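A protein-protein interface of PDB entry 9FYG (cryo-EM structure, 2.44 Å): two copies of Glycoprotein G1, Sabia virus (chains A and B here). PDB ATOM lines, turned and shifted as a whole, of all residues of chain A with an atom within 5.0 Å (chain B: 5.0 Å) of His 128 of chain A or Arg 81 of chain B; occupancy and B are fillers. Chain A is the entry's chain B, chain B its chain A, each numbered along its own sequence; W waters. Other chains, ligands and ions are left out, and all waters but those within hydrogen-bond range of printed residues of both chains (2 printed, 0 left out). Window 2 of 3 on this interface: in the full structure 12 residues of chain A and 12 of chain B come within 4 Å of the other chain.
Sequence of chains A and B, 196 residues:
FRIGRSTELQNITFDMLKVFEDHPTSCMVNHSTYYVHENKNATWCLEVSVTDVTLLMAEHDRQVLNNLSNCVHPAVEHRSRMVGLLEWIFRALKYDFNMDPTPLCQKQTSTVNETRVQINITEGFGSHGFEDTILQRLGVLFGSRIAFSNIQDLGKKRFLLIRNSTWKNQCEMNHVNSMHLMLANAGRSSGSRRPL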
ATOM      1  N   GLY A 126       4.069  21.355  17.412  1.00  0.00           N
ATOM      2  CA  GLY A 126       3.289  20.679  18.421  1.00  0.00           C
ATOM      3  C   GLY A 126       1.836  20.535  18.005  1.00  0.00           C
ATOM      4  O   GLY A 126       1.453  20.773  16.858  1.00  0.00           O
ATOM      5  N   SER A 127       1.016  20.132  18.967  1.00  0.00           N
ATOM      6  CA  SER A 127      -0.414  20.069  18.728  1.00  0.00           C
ATOM      7  C   SER A 127      -0.988  21.478  18.634  1.00  0.00           C
ATOM      8  O   SER A 127      -0.349  22.464  19.014  1.00  0.00           O
ATOM      9  CB  SER A 127      -1.111  19.278  19.832  1.00  0.00           C
ATOM     10  OG  SER A 127      -1.154  20.011  21.043  1.00  0.00           O
ATOM     11  N   HIS A 128      -2.206  21.567  18.106  1.00  0.00           N
ATOM     12  CA  HIS A 128      -2.861  22.860  17.967  1.00  0.00           C
ATOM     13  C   HIS A 128      -3.016  23.530  19.326  1.00  0.00           C
ATOM     14  O   HIS A 128      -3.455  22.906  20.296  1.00  0.00           O
ATOM     15  CB  HIS A 128      -4.224  22.686  17.299  1.00  0.00           C
ATOM     16  CG  HIS A 128      -4.981  23.965  17.128  1.00  0.00           C
ATOM     17  ND1 HIS A 128      -5.813  24.472  18.104  1.00  0.00           N
ATOM     18  CD2 HIS A 128      -5.032  24.840  16.097  1.00  0.00           C
ATOM     19  CE1 HIS A 128      -6.341  25.606  17.681  1.00  0.00           C
ATOM     20  NE2 HIS A 128      -5.882  25.851  16.467  1.00  0.00           N
ATOM     21  N   GLY A 129      -2.642  24.806  19.396  1.00  0.00           N
ATOM     22  CA  GLY A 129      -2.749  25.575  20.616  1.00  0.00           C
ATOM     23  C   GLY A 129      -1.598  25.433  21.588  1.00  0.00           C
ATOM     24  O   GLY A 129      -1.640  26.051  22.658  1.00  0.00           O
ATOM     25  N   PHE A 130      -0.578  24.637  21.262  1.00  0.00           N
ATOM     26  CA  PHE A 130       0.552  24.465  22.173  1.00  0.00           C
ATOM     27  C   PHE A 130       1.338  25.762  22.337  1.00  0.00           C
ATOM     28  O   PHE A 130       1.734  26.119  23.455  1.00  0.00           O
ATOM     29  CB  PHE A 130       1.461  23.343  21.672  1.00  0.00           C
ATOM     30  CG  PHE A 130       2.808  23.316  22.332  1.00  0.00           C
ATOM     31  CD1 PHE A 130       2.947  22.885  23.640  1.00  0.00           C
ATOM     32  CD2 PHE A 130       3.937  23.727  21.644  1.00  0.00           C
ATOM     33  CE1 PHE A 130       4.184  22.865  24.249  1.00  0.00           C
ATOM     34  CE2 PHE A 130       5.176  23.707  22.248  1.00  0.00           C
ATOM     35  CZ  PHE A 130       5.299  23.277  23.553  1.00  0.00           C
ATOM     36  N   GLU B  38     -14.297  18.889  19.147  1.00  0.00           N
ATOM     37  CA  GLU B  38     -13.404  20.023  19.388  1.00  0.00           C
ATOM     38  C   GLU B  38     -14.189  21.302  19.638  1.00  0.00           C
ATOM     39  O   GLU B  38     -13.928  22.030  20.602  1.00  0.00           O
ATOM     40  CB  GLU B  38     -12.463  20.234  18.205  1.00  0.00           C
ATOM     41  CG  GLU B  38     -11.472  21.355  18.463  1.00  0.00           C
ATOM     42  CD  GLU B  38     -10.577  21.650  17.287  1.00  0.00           C
ATOM     43  OE1 GLU B  38     -10.762  21.028  16.222  1.00  0.00           O
ATOM     44  OE2 GLU B  38      -9.681  22.506  17.432  1.00  0.00           O
ATOM     45  N   ASN B  39     -15.135  21.602  18.761  1.00  0.00           N
ATOM     46  CA  ASN B  39     -16.025  22.741  18.919  1.00  0.00           C
ATOM     47  C   ASN B  39     -17.271  22.451  18.094  1.00  0.00           C
ATOM     48  O   ASN B  39     -17.373  21.411  17.440  1.00  0.00           O
ATOM     49  CB  ASN B  39     -15.339  24.055  18.526  1.00  0.00           C
ATOM     50  CG  ASN B  39     -14.785  24.033  17.115  1.00  0.00           C
ATOM     51  OD1 ASN B  39     -15.533  24.050  16.141  1.00  0.00           O
ATOM     52  ND2 ASN B  39     -13.463  24.012  17.000  1.00  0.00           N
ATOM     53  N   TRP B  44     -15.408  16.695  12.335  1.00  0.00           N
ATOM     54  CA  TRP B  44     -14.878  15.436  12.828  1.00  0.00           C
ATOM     55  C   TRP B  44     -15.055  15.370  14.340  1.00  0.00           C
ATOM     56  O   TRP B  44     -15.451  16.341  14.988  1.00  0.00           O
ATOM     57  CB  TRP B  44     -13.399  15.286  12.455  1.00  0.00           C
ATOM     58  CG  TRP B  44     -12.573  16.411  12.982  1.00  0.00           C
ATOM     59  CD1 TRP B  44     -12.404  17.638  12.415  1.00  0.00           C
ATOM     60  CD2 TRP B  44     -11.831  16.428  14.204  1.00  0.00           C
ATOM     61  NE1 TRP B  44     -11.591  18.415  13.200  1.00  0.00           N
ATOM     62  CE2 TRP B  44     -11.224  17.695  14.305  1.00  0.00           C
ATOM     63  CE3 TRP B  44     -11.613  15.493  15.218  1.00  0.00           C
ATOM     64  CZ2 TRP B  44     -10.416  18.049  15.381  1.00  0.00           C
ATOM     65  CZ3 TRP B  44     -10.810  15.845  16.282  1.00  0.00           C
ATOM     66  CH2 TRP B  44     -10.223  17.114  16.358  1.00  0.00           C
ATOM     67  N   HIS B  78      -7.000  18.572   9.637  1.00  0.00           N
ATOM     68  CA  HIS B  78      -7.146  18.890  11.051  1.00  0.00           C
ATOM     69  C   HIS B  78      -6.218  18.062  11.928  1.00  0.00           C
ATOM     70  O   HIS B  78      -6.558  17.770  13.080  1.00  0.00           O
ATOM     71  CB  HIS B  78      -8.601  18.700  11.479  1.00  0.00           C
ATOM     72  CG  HIS B  78      -9.193  17.402  11.028  1.00  0.00           C
ATOM     73  ND1 HIS B  78      -9.714  17.219   9.765  1.00  0.00           N
ATOM     74  CD2 HIS B  78      -9.341  16.219  11.671  1.00  0.00           C
ATOM     75  CE1 HIS B  78     -10.160  15.980   9.650  1.00  0.00           C
ATOM     76  NE2 HIS B  78      -9.945  15.353  10.793  1.00  0.00           N
ATOM     77  N   ARG B  79      -5.054  17.671  11.403  1.00  0.00           N
ATOM     78  CA  ARG B  79      -4.159  16.781  12.134  1.00  0.00           C
ATOM     79  C   ARG B  79      -3.717  17.390  13.459  1.00  0.00           C
ATOM     80  O   ARG B  79      -3.712  16.711  14.492  1.00  0.00           O
ATOM     81  CB  ARG B  79      -2.946  16.445  11.270  1.00  0.00           C
ATOM     82  CG  ARG B  79      -1.974  15.485  11.918  1.00  0.00           C
ATOM     83  CD  ARG B  79      -0.638  15.482  11.211  1.00  0.00           C
ATOM     84  NE  ARG B  79       0.368  14.755  11.973  1.00  0.00           N
ATOM     85  CZ  ARG B  79       1.118  15.293  12.924  1.00  0.00           C
ATOM     86  NH1 ARG B  79       1.000  16.568  13.260  1.00  0.00           N
ATOM     87  NH2 ARG B  79       2.008  14.534  13.558  1.00  0.00           N
ATOM     88  N   SER B  80      -3.342  18.670  13.447  1.00  0.00           N
ATOM     89  CA  SER B  80      -2.881  19.317  14.670  1.00  0.00           C
ATOM     90  C   SER B  80      -3.994  19.385  15.710  1.00  0.00           C
ATOM     91  O   SER B  80      -3.768  19.106  16.894  1.00  0.00           O
ATOM     92  CB  SER B  80      -2.350  20.712  14.344  1.00  0.00           C
ATOM     93  OG  SER B  80      -1.595  21.239  15.415  1.00  0.00           O
ATOM     94  N   ARG B  81      -5.209  19.729  15.280  1.00  0.00           N
ATOM     95  CA  ARG B  81      -6.341  19.771  16.197  1.00  0.00           C
ATOM     96  C   ARG B  81      -6.708  18.376  16.689  1.00  0.00           C
ATOM     97  O   ARG B  81      -7.117  18.207  17.842  1.00  0.00           O
ATOM     98  CB  ARG B  81      -7.534  20.441  15.520  1.00  0.00           C
ATOM     99  CG  ARG B  81      -7.297  21.894  15.154  1.00  0.00           C
ATOM    100  CD  ARG B  81      -8.465  22.468  14.377  1.00  0.00           C
ATOM    101  NE  ARG B  81      -8.344  23.910  14.192  1.00  0.00           N
ATOM    102  CZ  ARG B  81      -8.748  24.814  15.073  1.00  0.00           C
ATOM    103  NH1 ARG B  81      -9.304  24.462  16.220  1.00  0.00           N
ATOM    104  NH2 ARG B  81      -8.590  26.104  14.796  1.00  0.00           N
ATOM    105  N   MET B  82      -6.569  17.364  15.830  1.00  0.00           N
ATOM    106  CA  MET B  82      -6.846  15.993  16.245  1.00  0.00           C
ATOM    107  C   MET B  82      -5.869  15.536  17.324  1.00  0.00           C
ATOM    108  O   MET B  82      -6.271  14.946  18.334  1.00  0.00           O
ATOM    109  CB  MET B  82      -6.783  15.065  15.035  1.00  0.00           C
ATOM    110  CG  MET B  82      -7.281  13.661  15.298  1.00  0.00           C
ATOM    111  SD  MET B  82      -7.611  12.805  13.754  1.00  0.00           S
ATOM    112  CE  MET B  82      -9.294  13.322  13.468  1.00  0.00           C
ATOM    113  N   VAL B  83      -4.577  15.803  17.122  1.00  0.00           N
ATOM    114  CA  VAL B  83      -3.575  15.450  18.124  1.00  0.00           C
ATOM    115  C   VAL B  83      -3.828  16.213  19.415  1.00  0.00           C
ATOM    116  O   VAL B  83      -3.733  15.655  20.519  1.00  0.00           O
ATOM    117  CB  VAL B  83      -2.159  15.711  17.578  1.00  0.00           C
ATOM    118  CG1 VAL B  83      -1.123  15.463  18.656  1.00  0.00           C
ATOM    119  CG2 VAL B  83      -1.889  14.839  16.367  1.00  0.00           C
ATOM    120  N   GLY B  84      -4.160  17.501  19.298  1.00  0.00           N
ATOM    121  CA  GLY B  84      -4.509  18.268  20.477  1.00  0.00           C
ATOM    122  C   GLY B  84      -5.651  17.643  21.252  1.00  0.00           C
ATOM    123  O   GLY B  84      -5.530  17.395  22.448  1.00  0.00           O
ATOM    124  N   LEU B  85      -6.751  17.322  20.562  1.00  0.00           N
ATOM    125  CA  LEU B  85      -7.916  16.756  21.235  1.00  0.00           C
ATOM    126  C   LEU B  85      -7.606  15.398  21.848  1.00  0.00           C
ATOM    127  O   LEU B  85      -8.139  15.062  22.913  1.00  0.00           O
ATOM    128  CB  LEU B  85      -9.089  16.647  20.260  1.00  0.00           C
ATOM    129  CG  LEU B  85     -10.472  16.441  20.884  1.00  0.00           C
ATOM    130  CD1 LEU B  85     -10.831  17.600  21.802  1.00  0.00           C
ATOM    131  CD2 LEU B  85     -11.531  16.250  19.817  1.00  0.00           C
ATOM    132  N   LEU B  86      -6.741  14.612  21.206  1.00  0.00           N
ATOM    133  CA  LEU B  86      -6.280  13.373  21.821  1.00  0.00           C
ATOM    134  C   LEU B  86      -5.555  13.649  23.134  1.00  0.00           C
ATOM    135  O   LEU B  86      -5.746  12.929  24.121  1.00  0.00           O
ATOM    136  CB  LEU B  86      -5.372  12.612  20.855  1.00  0.00           C
ATOM    137  CG  LEU B  86      -6.040  11.556  19.977  1.00  0.00           C
ATOM    138  CD1 LEU B  86      -5.066  11.045  18.928  1.00  0.00           C
ATOM    139  CD2 LEU B  86      -6.581  10.412  20.818  1.00  0.00           C
ATOM    140  N   SER B 192     -11.840  29.591  19.849  1.00  0.00           N
ATOM    141  CA  SER B 192     -11.508  30.384  18.670  1.00  0.00           C
ATOM    142  C   SER B 192     -12.721  31.168  18.182  1.00  0.00           C
ATOM    143  O   SER B 192     -13.711  30.584  17.741  1.00  0.00           O
ATOM    144  CB  SER B 192     -10.975  29.487  17.551  1.00  0.00           C
ATOM    145  OG  SER B 192      -9.718  28.932  17.897  1.00  0.00           O
HETATM  146  O   HOH W   1       0.173  17.948  15.857  1.00  0.00           O
HETATM  147  O   HOH W   2       0.089  23.897  16.098  1.00  0.00           O
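The side-chain hydroxyl (OG) of Ser 80 of chain B is in hydrogen-bond range of the backbone carbonyl oxygen (O) of Gly 126 of chain A (3.4 Å). N of His 128 of chain A sits at hydrogen-bond distance from OG of Ser 80 of chain B (2.8 Å). NE2 of His 128 of chain A lies within hydrogen-bond range of NH2 of Arg 81 of chain B (3.2 Å).
OE1 of Glu 38 of chain B lies within salt-bridge range of NH1 of Arg 81 of chain B (3.7 Å).
Among the printed residues, merely in contact across the chains: Ser 127 of chain A with Ser 80 of chain B, Ser 127 of chain A with Gly 84 of chain B and Ser 127 of chain A with Val 83 of chain B.
Of chain B, only Ser 80 and Arg 81 come within 4 Å of His 128 of chain A. Glu 38 of chain B touches none of the printed residues of chain A. Trp 44 of chain B touches none of the printed residues of chain A. Arg 81 of chain B touches just one residue of chain A: His 128. Of the printed residues of chain A, Val 83 of chain B touches Ser 127. Printed residues of chain A within 4 Å of Gly 84 of chain B: Ser 127 (3.6 Å).
Printed residues of chain B that touch a printed residue of chain A: Ser 80, Arg 81, Val 83 and Gly 84. Hydrophobic or aromatic side chains of chain B that line the printed part of chain A: Val 83. Of the 5 printed residues of chain A, 3 touch a printed residue of chain B. Hydrophobic or aromatic side chains of chain A within 4 Å of the printed part of chain B: His 128. Among the printed residues, 6 pairs touch across the chains.
No position is printed for both chains. Of the 6 pairs that touch across the chains among the printed residues, none has its exchanged pair printed and touching as well.
Water W1 lies within hydrogen-bond range of NH1 of Arg 79 of chain B and O of Gly 126 of chain A. Water W2 lies within hydrogen-bond range of OG of Ser 80 of chain B, O of Ser 127 of chain A and O of Gly 126 of chain A.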
